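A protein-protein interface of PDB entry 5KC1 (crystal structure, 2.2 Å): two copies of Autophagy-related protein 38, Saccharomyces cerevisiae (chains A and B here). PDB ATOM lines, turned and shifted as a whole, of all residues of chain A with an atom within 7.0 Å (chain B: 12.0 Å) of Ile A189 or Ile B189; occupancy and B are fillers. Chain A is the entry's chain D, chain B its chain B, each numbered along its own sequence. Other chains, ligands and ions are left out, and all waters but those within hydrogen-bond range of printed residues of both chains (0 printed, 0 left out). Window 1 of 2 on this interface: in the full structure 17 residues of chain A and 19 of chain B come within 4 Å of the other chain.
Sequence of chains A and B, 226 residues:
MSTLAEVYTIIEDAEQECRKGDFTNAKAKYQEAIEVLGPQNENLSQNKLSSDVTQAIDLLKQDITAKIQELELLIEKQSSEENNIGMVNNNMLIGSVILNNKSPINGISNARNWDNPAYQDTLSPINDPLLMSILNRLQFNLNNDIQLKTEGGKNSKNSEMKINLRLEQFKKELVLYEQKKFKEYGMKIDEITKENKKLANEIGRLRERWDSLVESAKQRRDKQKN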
ATOM      1  N   LYS A 183     -31.324  22.397  -3.173  1.00  0.00           N
ATOM      2  CA  LYS A 183     -30.525  22.220  -4.385  1.00  0.00           C
ATOM      3  C   LYS A 183     -29.054  21.984  -4.064  1.00  0.00           C
ATOM      4  O   LYS A 183     -28.449  21.034  -4.563  1.00  0.00           O
ATOM      5  CB  LYS A 183     -30.645  23.438  -5.303  1.00  0.00           C
ATOM      6  CG  LYS A 183     -32.054  23.762  -5.752  1.00  0.00           C
ATOM      7  CD  LYS A 183     -32.095  25.107  -6.467  1.00  0.00           C
ATOM      8  CE  LYS A 183     -33.528  25.574  -6.683  1.00  0.00           C
ATOM      9  NZ  LYS A 183     -33.582  27.013  -7.056  1.00  0.00           N
ATOM     10  N   GLU A 184     -28.483  22.860  -3.238  1.00  0.00           N
ATOM     11  CA  GLU A 184     -27.068  22.779  -2.882  1.00  0.00           C
ATOM     12  C   GLU A 184     -26.706  21.435  -2.255  1.00  0.00           C
ATOM     13  O   GLU A 184     -25.625  20.902  -2.499  1.00  0.00           O
ATOM     14  CB  GLU A 184     -26.686  23.907  -1.919  1.00  0.00           C
ATOM     15  CG  GLU A 184     -26.949  25.314  -2.437  1.00  0.00           C
ATOM     16  CD  GLU A 184     -26.669  26.369  -1.379  1.00  0.00           C
ATOM     17  OE1 GLU A 184     -26.121  26.011  -0.318  1.00  0.00           O
ATOM     18  OE2 GLU A 184     -26.994  27.552  -1.603  1.00  0.00           O
ATOM     19  N   TYR A 185     -27.607  20.895  -1.443  1.00  0.00           N
ATOM     20  CA  TYR A 185     -27.373  19.608  -0.800  1.00  0.00           C
ATOM     21  C   TYR A 185     -27.570  18.467  -1.790  1.00  0.00           C
ATOM     22  O   TYR A 185     -26.867  17.458  -1.738  1.00  0.00           O
ATOM     23  CB  TYR A 185     -28.296  19.424   0.412  1.00  0.00           C
ATOM     24  CG  TYR A 185     -27.723  19.931   1.722  1.00  0.00           C
ATOM     25  CD1 TYR A 185     -26.820  19.167   2.448  1.00  0.00           C
ATOM     26  CD2 TYR A 185     -28.095  21.167   2.238  1.00  0.00           C
ATOM     27  CE1 TYR A 185     -26.298  19.618   3.642  1.00  0.00           C
ATOM     28  CE2 TYR A 185     -27.573  21.630   3.436  1.00  0.00           C
ATOM     29  CZ  TYR A 185     -26.676  20.850   4.134  1.00  0.00           C
ATOM     30  OH  TYR A 185     -26.150  21.297   5.326  1.00  0.00           O
ATOM     31  N   GLY A 186     -28.534  18.633  -2.692  1.00  0.00           N
ATOM     32  CA  GLY A 186     -28.822  17.622  -3.692  1.00  0.00           C
ATOM     33  C   GLY A 186     -27.658  17.397  -4.638  1.00  0.00           C
ATOM     34  O   GLY A 186     -27.208  16.268  -4.828  1.00  0.00           O
ATOM     35  N   MET A 187     -27.170  18.480  -5.232  1.00  0.00           N
ATOM     36  CA  MET A 187     -26.044  18.409  -6.156  1.00  0.00           C
ATOM     37  C   MET A 187     -24.814  17.793  -5.506  1.00  0.00           C
ATOM     38  O   MET A 187     -24.146  16.949  -6.101  1.00  0.00           O
ATOM     39  CB  MET A 187     -25.702  19.799  -6.686  1.00  0.00           C
ATOM     40  CG  MET A 187     -26.820  20.459  -7.470  1.00  0.00           C
ATOM     41  SD  MET A 187     -26.284  22.016  -8.200  1.00  0.00           S
ATOM     42  CE  MET A 187     -25.488  22.791  -6.793  1.00  0.00           C
ATOM     43  N   LYS A 188     -24.520  18.221  -4.283  1.00  0.00           N
ATOM     44  CA  LYS A 188     -23.339  17.747  -3.573  1.00  0.00           C
ATOM     45  C   LYS A 188     -23.462  16.270  -3.231  1.00  0.00           C
ATOM     46  O   LYS A 188     -22.468  15.550  -3.187  1.00  0.00           O
ATOM     47  CB  LYS A 188     -23.114  18.563  -2.302  1.00  0.00           C
ATOM     48  CG  LYS A 188     -21.760  18.337  -1.652  1.00  0.00           C
ATOM     49  CD  LYS A 188     -20.635  18.807  -2.558  1.00  0.00           C
ATOM     50  CE  LYS A 188     -19.310  18.864  -1.813  1.00  0.00           C
ATOM     51  NZ  LYS A 188     -19.327  19.880  -0.721  1.00  0.00           N
ATOM     52  N   ILE A 189     -24.686  15.822  -2.984  1.00  0.00           N
ATOM     53  CA  ILE A 189     -24.924  14.420  -2.667  1.00  0.00           C
ATOM     54  C   ILE A 189     -24.773  13.557  -3.914  1.00  0.00           C
ATOM     55  O   ILE A 189     -24.208  12.467  -3.858  1.00  0.00           O
ATOM     56  CB  ILE A 189     -26.321  14.202  -2.054  1.00  0.00           C
ATOM     57  CG1 ILE A 189     -26.334  14.660  -0.592  1.00  0.00           C
ATOM     58  CG2 ILE A 189     -26.716  12.741  -2.141  1.00  0.00           C
ATOM     59  CD1 ILE A 189     -27.691  14.532   0.085  1.00  0.00           C
ATOM     60  N   ASP A 190     -25.274  14.053  -5.040  1.00  0.00           N
ATOM     61  CA  ASP A 190     -25.173  13.326  -6.299  1.00  0.00           C
ATOM     62  C   ASP A 190     -23.737  13.304  -6.803  1.00  0.00           C
ATOM     63  O   ASP A 190     -23.252  12.282  -7.286  1.00  0.00           O
ATOM     64  CB  ASP A 190     -26.094  13.945  -7.353  1.00  0.00           C
ATOM     65  CG  ASP A 190     -27.557  13.717  -7.048  1.00  0.00           C
ATOM     66  OD1 ASP A 190     -27.876  12.695  -6.404  1.00  0.00           O
ATOM     67  OD2 ASP A 190     -28.389  14.557  -7.450  1.00  0.00           O
ATOM     68  N   GLU A 191     -23.065  14.443  -6.682  1.00  0.00           N
ATOM     69  CA  GLU A 191     -21.681  14.578  -7.113  1.00  0.00           C
ATOM     70  C   GLU A 191     -20.762  13.595  -6.398  1.00  0.00           C
ATOM     71  O   GLU A 191     -19.775  13.133  -6.965  1.00  0.00           O
ATOM     72  CB  GLU A 191     -21.199  16.009  -6.876  1.00  0.00           C
ATOM     73  CG  GLU A 191     -19.723  16.226  -7.131  1.00  0.00           C
ATOM     74  CD  GLU A 191     -19.304  17.659  -6.876  1.00  0.00           C
ATOM     75  OE1 GLU A 191     -20.180  18.482  -6.528  1.00  0.00           O
ATOM     76  OE2 GLU A 191     -18.101  17.963  -7.023  1.00  0.00           O
ATOM     77  N   ILE A 192     -21.093  13.275  -5.153  1.00  0.00           N
ATOM     78  CA  ILE A 192     -20.260  12.397  -4.340  1.00  0.00           C
ATOM     79  C   ILE A 192     -20.673  10.934  -4.485  1.00  0.00           C
ATOM     80  O   ILE A 192     -19.879  10.031  -4.222  1.00  0.00           O
ATOM     81  CB  ILE A 192     -20.307  12.806  -2.854  1.00  0.00           C
ATOM     82  CG1 ILE A 192     -19.665  14.180  -2.670  1.00  0.00           C
ATOM     83  CG2 ILE A 192     -19.585  11.791  -1.987  1.00  0.00           C
ATOM     84  CD1 ILE A 192     -19.502  14.585  -1.223  1.00  0.00           C
ATOM     85  N   THR A 193     -21.910  10.697  -4.905  1.00  0.00           N
ATOM     86  CA  THR A 193     -22.343   9.338  -5.201  1.00  0.00           C
ATOM     87  C   THR A 193     -21.726   8.886  -6.520  1.00  0.00           C
ATOM     88  O   THR A 193     -21.307   7.737  -6.655  1.00  0.00           O
ATOM     89  CB  THR A 193     -23.875   9.216  -5.276  1.00  0.00           C
ATOM     90  OG1 THR A 193     -24.388  10.165  -6.219  1.00  0.00           O
ATOM     91  CG2 THR A 193     -24.498   9.467  -3.911  1.00  0.00           C
ATOM     92  N   LYS A 194     -21.663   9.798  -7.486  1.00  0.00           N
ATOM     93  CA  LYS A 194     -21.020   9.512  -8.763  1.00  0.00           C
ATOM     94  C   LYS A 194     -19.538   9.215  -8.558  1.00  0.00           C
ATOM     95  O   LYS A 194     -19.033   8.191  -9.016  1.00  0.00           O
ATOM     96  CB  LYS A 194     -21.196  10.680  -9.735  1.00  0.00           C
ATOM     97  CG  LYS A 194     -22.645  10.976 -10.085  1.00  0.00           C
ATOM     98  CD  LYS A 194     -22.760  12.182 -10.998  1.00  0.00           C
ATOM     99  CE  LYS A 194     -24.215  12.522 -11.280  1.00  0.00           C
ATOM    100  NZ  LYS A 194     -24.349  13.709 -12.170  1.00  0.00           N
ATOM    101  N   GLN B 179     -30.698  24.752  10.789  1.00  0.00           N
ATOM    102  CA  GLN B 179     -29.614  23.806  11.039  1.00  0.00           C
ATOM    103  C   GLN B 179     -30.142  22.395  11.278  1.00  0.00           C
ATOM    104  O   GLN B 179     -29.612  21.429  10.732  1.00  0.00           O
ATOM    105  CB  GLN B 179     -28.774  24.252  12.232  1.00  0.00           C
ATOM    106  CG  GLN B 179     -27.701  23.258  12.649  1.00  0.00           C
ATOM    107  CD  GLN B 179     -26.458  23.317  11.771  1.00  0.00           C
ATOM    108  OE1 GLN B 179     -26.445  23.971  10.725  1.00  0.00           O
ATOM    109  NE2 GLN B 179     -25.399  22.637  12.203  1.00  0.00           N
ATOM    110  N   LYS B 181     -33.177  21.288  10.383  1.00  0.00           N
ATOM    111  CA  LYS B 181     -33.938  20.875   9.206  1.00  0.00           C
ATOM    112  C   LYS B 181     -33.082  20.159   8.161  1.00  0.00           C
ATOM    113  O   LYS B 181     -33.534  19.203   7.530  1.00  0.00           O
ATOM    114  CB  LYS B 181     -34.613  22.090   8.568  1.00  0.00           C
ATOM    115  CG  LYS B 181     -35.291  21.813   7.240  1.00  0.00           C
ATOM    116  CD  LYS B 181     -36.167  22.984   6.839  1.00  0.00           C
ATOM    117  CE  LYS B 181     -36.780  22.781   5.459  1.00  0.00           C
ATOM    118  NZ  LYS B 181     -37.717  21.627   5.412  1.00  0.00           N
ATOM    119  N   PHE B 182     -31.849  20.626   7.977  1.00  0.00           N
ATOM    120  CA  PHE B 182     -30.969  20.074   6.946  1.00  0.00           C
ATOM    121  C   PHE B 182     -29.871  19.189   7.514  1.00  0.00           C
ATOM    122  O   PHE B 182     -28.908  18.881   6.816  1.00  0.00           O
ATOM    123  CB  PHE B 182     -30.333  21.200   6.123  1.00  0.00           C
ATOM    124  CG  PHE B 182     -31.317  21.973   5.295  1.00  0.00           C
ATOM    125  CD1 PHE B 182     -31.780  21.465   4.093  1.00  0.00           C
ATOM    126  CD2 PHE B 182     -31.777  23.210   5.718  1.00  0.00           C
ATOM    127  CE1 PHE B 182     -32.702  22.173   3.323  1.00  0.00           C
ATOM    128  CE2 PHE B 182     -32.690  23.925   4.962  1.00  0.00           C
ATOM    129  CZ  PHE B 182     -33.157  23.406   3.760  1.00  0.00           C
ATOM    130  N   LYS B 183     -30.022  18.775   8.770  1.00  0.00           N
ATOM    131  CA  LYS B 183     -28.972  18.031   9.471  1.00  0.00           C
ATOM    132  C   LYS B 183     -28.741  16.638   8.885  1.00  0.00           C
ATOM    133  O   LYS B 183     -27.609  16.166   8.838  1.00  0.00           O
ATOM    134  CB  LYS B 183     -29.304  17.910  10.961  1.00  0.00           C
ATOM    135  CG  LYS B 183     -28.184  17.310  11.794  1.00  0.00           C
ATOM    136  CD  LYS B 183     -28.556  17.265  13.268  1.00  0.00           C
ATOM    137  CE  LYS B 183     -27.394  16.777  14.122  1.00  0.00           C
ATOM    138  NZ  LYS B 183     -27.757  16.691  15.565  1.00  0.00           N
ATOM    139  N   GLU B 184     -29.811  15.987   8.436  1.00  0.00           N
ATOM    140  CA  GLU B 184     -29.702  14.642   7.872  1.00  0.00           C
ATOM    141  C   GLU B 184     -28.978  14.644   6.526  1.00  0.00           C
ATOM    142  O   GLU B 184     -28.323  13.671   6.163  1.00  0.00           O
ATOM    143  CB  GLU B 184     -31.085  14.011   7.720  1.00  0.00           C
ATOM    144  CG  GLU B 184     -32.024  14.786   6.817  1.00  0.00           C
ATOM    145  CD  GLU B 184     -33.417  14.189   6.784  1.00  0.00           C
ATOM    146  OE1 GLU B 184     -34.276  14.718   6.047  1.00  0.00           O
ATOM    147  OE2 GLU B 184     -33.654  13.190   7.496  1.00  0.00           O
ATOM    148  N   TYR B 185     -29.104  15.740   5.787  1.00  0.00           N
ATOM    149  CA  TYR B 185     -28.387  15.893   4.528  1.00  0.00           C
ATOM    150  C   TYR B 185     -26.905  16.105   4.800  1.00  0.00           C
ATOM    151  O   TYR B 185     -26.050  15.601   4.073  1.00  0.00           O
ATOM    152  CB  TYR B 185     -28.953  17.060   3.716  1.00  0.00           C
ATOM    153  CG  TYR B 185     -30.389  16.866   3.287  1.00  0.00           C
ATOM    154  CD1 TYR B 185     -31.439  17.183   4.138  1.00  0.00           C
ATOM    155  CD2 TYR B 185     -30.696  16.365   2.030  1.00  0.00           C
ATOM    156  CE1 TYR B 185     -32.751  17.002   3.752  1.00  0.00           C
ATOM    157  CE2 TYR B 185     -32.002  16.185   1.633  1.00  0.00           C
ATOM    158  CZ  TYR B 185     -33.028  16.503   2.497  1.00  0.00           C
ATOM    159  OH  TYR B 185     -34.335  16.323   2.098  1.00  0.00           O
ATOM    160  N   GLY B 186     -26.605  16.851   5.858  1.00  0.00           N
ATOM    161  CA  GLY B 186     -25.229  17.108   6.233  1.00  0.00           C
ATOM    162  C   GLY B 186     -24.534  15.847   6.701  1.00  0.00           C
ATOM    163  O   GLY B 186     -23.324  15.695   6.535  1.00  0.00           O
ATOM    164  N   MET B 187     -25.307  14.939   7.289  1.00  0.00           N
ATOM    165  CA  MET B 187     -24.777  13.665   7.759  1.00  0.00           C
ATOM    166  C   MET B 187     -24.580  12.694   6.600  1.00  0.00           C
ATOM    167  O   MET B 187     -23.588  11.968   6.552  1.00  0.00           O
ATOM    168  CB  MET B 187     -25.703  13.047   8.811  1.00  0.00           C
ATOM    169  CG  MET B 187     -25.702  13.776  10.147  1.00  0.00           C
ATOM    170  SD  MET B 187     -26.610  12.895  11.434  1.00  0.00           S
ATOM    171  CE  MET B 187     -28.254  12.818  10.721  1.00  0.00           C
ATOM    172  N   LYS B 188     -25.536  12.683   5.675  1.00  0.00           N
ATOM    173  CA  LYS B 188     -25.445  11.855   4.479  1.00  0.00           C
ATOM    174  C   LYS B 188     -24.142  12.142   3.745  1.00  0.00           C
ATOM    175  O   LYS B 188     -23.415  11.226   3.363  1.00  0.00           O
ATOM    176  CB  LYS B 188     -26.639  12.107   3.557  1.00  0.00           C
ATOM    177  CG  LYS B 188     -26.715  11.186   2.346  1.00  0.00           C
ATOM    178  CD  LYS B 188     -27.239   9.808   2.728  1.00  0.00           C
ATOM    179  CE  LYS B 188     -27.625   9.001   1.496  1.00  0.00           C
ATOM    180  NZ  LYS B 188     -28.297   7.719   1.857  1.00  0.00           N
ATOM    181  N   ILE B 189     -23.853  13.426   3.563  1.00  0.00           N
ATOM    182  CA  ILE B 189     -22.608  13.862   2.941  1.00  0.00           C
ATOM    183  C   ILE B 189     -21.385  13.355   3.691  1.00  0.00           C
ATOM    184  O   ILE B 189     -20.387  12.980   3.080  1.00  0.00           O
ATOM    185  CB  ILE B 189     -22.529  15.398   2.861  1.00  0.00           C
ATOM    186  CG1 ILE B 189     -23.491  15.927   1.798  1.00  0.00           C
ATOM    187  CG2 ILE B 189     -21.108  15.846   2.568  1.00  0.00           C
ATOM    188  CD1 ILE B 189     -23.431  17.429   1.615  1.00  0.00           C
ATOM    189  N   ASP B 190     -21.464  13.345   5.018  1.00  0.00           N
ATOM    190  CA  ASP B 190     -20.315  12.969   5.836  1.00  0.00           C
ATOM    191  C   ASP B 190     -20.022  11.476   5.753  1.00  0.00           C
ATOM    192  O   ASP B 190     -18.864  11.072   5.648  1.00  0.00           O
ATOM    193  CB  ASP B 190     -20.535  13.377   7.295  1.00  0.00           C
ATOM    194  CG  ASP B 190     -20.663  14.880   7.469  1.00  0.00           C
ATOM    195  OD1 ASP B 190     -20.236  15.628   6.562  1.00  0.00           O
ATOM    196  OD2 ASP B 190     -21.192  15.315   8.514  1.00  0.00           O
ATOM    197  N   GLU B 191     -21.070  10.658   5.794  1.00  0.00           N
ATOM    198  CA  GLU B 191     -20.893   9.211   5.782  1.00  0.00           C
ATOM    199  C   GLU B 191     -20.428   8.727   4.413  1.00  0.00           C
ATOM    200  O   GLU B 191     -19.569   7.850   4.316  1.00  0.00           O
ATOM    201  CB  GLU B 191     -22.185   8.496   6.185  1.00  0.00           C
ATOM    202  CG  GLU B 191     -23.336   8.667   5.207  1.00  0.00           C
ATOM    203  CD  GLU B 191     -24.525   7.790   5.555  1.00  0.00           C
ATOM    204  OE1 GLU B 191     -24.317   6.594   5.853  1.00  0.00           O
ATOM    205  OE2 GLU B 191     -25.666   8.298   5.539  1.00  0.00           O
ATOM    206  N   ILE B 192     -20.998   9.305   3.360  1.00  0.00           N
ATOM    207  CA  ILE B 192     -20.623   8.941   1.999  1.00  0.00           C
ATOM    208  C   ILE B 192     -19.227   9.449   1.662  1.00  0.00           C
ATOM    209  O   ILE B 192     -18.460   8.774   0.979  1.00  0.00           O
ATOM    210  CB  ILE B 192     -21.622   9.488   0.974  1.00  0.00           C
ATOM    211  CG1 ILE B 192     -22.954   8.746   1.095  1.00  0.00           C
ATOM    212  CG2 ILE B 192     -21.068   9.350  -0.428  1.00  0.00           C
ATOM    213  CD1 ILE B 192     -23.964   9.130   0.040  1.00  0.00           C
ATOM    214  N   THR B 193     -18.900  10.641   2.150  1.00  0.00           N
ATOM    215  CA  THR B 193     -17.563  11.192   1.982  1.00  0.00           C
ATOM    216  C   THR B 193     -16.551  10.332   2.726  1.00  0.00           C
ATOM    217  O   THR B 193     -15.361  10.346   2.417  1.00  0.00           O
ATOM    218  CB  THR B 193     -17.477  12.643   2.486  1.00  0.00           C
ATOM    219  OG1 THR B 193     -18.441  13.448   1.796  1.00  0.00           O
ATOM    220  CG2 THR B 193     -16.089  13.211   2.246  1.00  0.00           C
ATOM    221  N   LYS B 194     -17.035   9.584   3.712  1.00  0.00           N
ATOM    222  CA  LYS B 194     -16.190   8.653   4.446  1.00  0.00           C
ATOM    223  C   LYS B 194     -15.958   7.398   3.615  1.00  0.00           C
ATOM    224  O   LYS B 194     -14.876   6.811   3.646  1.00  0.00           O
ATOM    225  CB  LYS B 194     -16.819   8.289   5.794  1.00  0.00           C
ATOM    226  CG  LYS B 194     -15.992   7.305   6.612  1.00  0.00           C
ATOM    227  CD  LYS B 194     -16.659   6.978   7.939  1.00  0.00           C
ATOM    228  CE  LYS B 194     -15.810   6.016   8.758  1.00  0.00           C
ATOM    229  NZ  LYS B 194     -16.441   5.691  10.067  1.00  0.00           N
ATOM    230  N   GLU B 195     -16.986   6.994   2.874  1.00  0.00           N
ATOM    231  CA  GLU B 195     -16.891   5.835   1.996  1.00  0.00           C
ATOM    232  C   GLU B 195     -15.880   6.088   0.883  1.00  0.00           C
ATOM    233  O   GLU B 195     -15.131   5.191   0.497  1.00  0.00           O
ATOM    234  CB  GLU B 195     -18.260   5.493   1.404  1.00  0.00           C
ATOM    235  CG  GLU B 195     -19.300   5.081   2.436  1.00  0.00           C
ATOM    236  CD  GLU B 195     -20.675   4.861   1.826  1.00  0.00           C
ATOM    237  OE1 GLU B 195     -20.856   5.175   0.630  1.00  0.00           O
ATOM    238  OE2 GLU B 195     -21.577   4.375   2.543  1.00  0.00           O
ATOM    239  N   ASN B 196     -15.858   7.315   0.372  1.00  0.00           N
ATOM    240  CA  ASN B 196     -14.909   7.685  -0.670  1.00  0.00           C
ATOM    241  C   ASN B 196     -13.476   7.668  -0.158  1.00  0.00           C
ATOM    242  O   ASN B 196     -12.543   7.372  -0.906  1.00  0.00           O
ATOM    243  CB  ASN B 196     -15.246   9.064  -1.237  1.00  0.00           C
ATOM    244  CG  ASN B 196     -16.468   9.039  -2.129  1.00  0.00           C
ATOM    245  OD1 ASN B 196     -17.241   8.082  -2.113  1.00  0.00           O
ATOM    246  ND2 ASN B 196     -16.649  10.093  -2.916  1.00  0.00           N
ATOM    247  N   LYS B 197     -13.305   7.991   1.119  1.00  0.00           N
ATOM    248  CA  LYS B 197     -11.994   7.921   1.751  1.00  0.00           C
ATOM    249  C   LYS B 197     -11.540   6.471   1.858  1.00  0.00           C
ATOM    250  O   LYS B 197     -10.385   6.150   1.581  1.00  0.00           O
ATOM    251  CB  LYS B 197     -12.025   8.566   3.136  1.00  0.00           C
ATOM    252  CG  LYS B 197     -12.242  10.068   3.136  1.00  0.00           C
ATOM    253  CD  LYS B 197     -12.664  10.539   4.518  1.00  0.00           C
ATOM    254  CE  LYS B 197     -11.804   9.900   5.599  1.00  0.00           C
ATOM    255  NZ  LYS B 197     -12.344  10.136   6.967  1.00  0.00           N
ATOM    256  N   LYS B 198     -12.462   5.601   2.259  1.00  0.00           N
ATOM    257  CA  LYS B 198     -12.168   4.181   2.417  1.00  0.00           C
ATOM    258  C   LYS B 198     -11.800   3.541   1.082  1.00  0.00           C
ATOM    259  O   LYS B 198     -10.831   2.787   0.993  1.00  0.00           O
ATOM    260  CB  LYS B 198     -13.360   3.450   3.041  1.00  0.00           C
ATOM    261  CG  LYS B 198     -13.651   3.846   4.484  1.00  0.00           C
ATOM    262  CD  LYS B 198     -14.767   2.995   5.074  1.00  0.00           C
ATOM    263  CE  LYS B 198     -15.028   3.344   6.534  1.00  0.00           C
ATOM    264  NZ  LYS B 198     -16.095   2.488   7.129  1.00  0.00           N
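The backbone carbonyl oxygen of Ile B192 lies close to the side-chain amide oxygen of Asn B196 (3.4 Å).
O of Ile A189 lies close to OG1 of Thr A193.
Tyr A185 touches Ile B189, but with the chains exchanged Ile A189 does not touch Tyr B185 (4.02 Å).
Ile B189 touches its own counterpart, Ile A189.
Ile A192 touches its own counterpart, Ile B192.
Ile A192 touches Thr B193, but with the chains exchanged Thr A193 does not touch Ile B192 (4.001 Å).
12 positions are printed for both chains.
ND2 of Asn B196 sits at hydrogen-bond distance from O of Ile A192 (3.5 Å).
Of the 12 printed residues of chain A, 4 touch a printed residue of chain B.
Hydrophobic or aromatic side chains of chain A that line the printed part of chain B: Tyr A185, Ile A189 and Ile A192.
Along chain A the printed residues that touch a printed residue of chain B span positions 185 to 192.
Hydrophobic or aromatic side chains of chain B within 4 Å of the printed part of chain A: Phe B182, Tyr B185, Ile B189 and Ile B192.
Among the printed residues, 9 pairs touch across the chains.
Among the printed residues, merely in contact across the chains: Tyr A185 with Phe B182, Tyr A185 with Tyr B185, Tyr A185 with Gly B186, Tyr A185 with Ile B189, Lys A188 with Ile B189, Ile A189 with Ile B189, Ile A192 with Ile B192 and Ile A192 with Thr B193.
Ile A189 touches one residue of chain B.
Ile B189 touches just these residues of chain A: Tyr A185, Lys A188 and Ile A189.
Tyr A185 touches just these residues of chain B: Phe B182, Tyr B185, Gly B186 and Ile B189.
Of chain B, only Ile B189 comes within 4 Å of Lys A188.
No residue of chain B comes within 4 Å of Asp A190.
Of chain B, only Ile B192 (3.3 Å), Thr B193 (3.4 Å) and Asn B196 (3.5 Å) come within 4 Å of Ile A192.
Printed residues of chain A within 4 Å of Gly B186: Tyr A185 (3.6 Å).
Printed residues of chain A within 4 Å of Thr B193: Ile A192 (3.4 Å).
Of the printed residues of chain A, Tyr B185 touches Tyr A185.
Of the printed residues of chain A, Phe B182 touches Tyr A185.
Lys A183 touches none of the printed residues of chain B.
The nearest residue of chain B that does not touch Ile A189 is Tyr B185 (4.02 Å).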
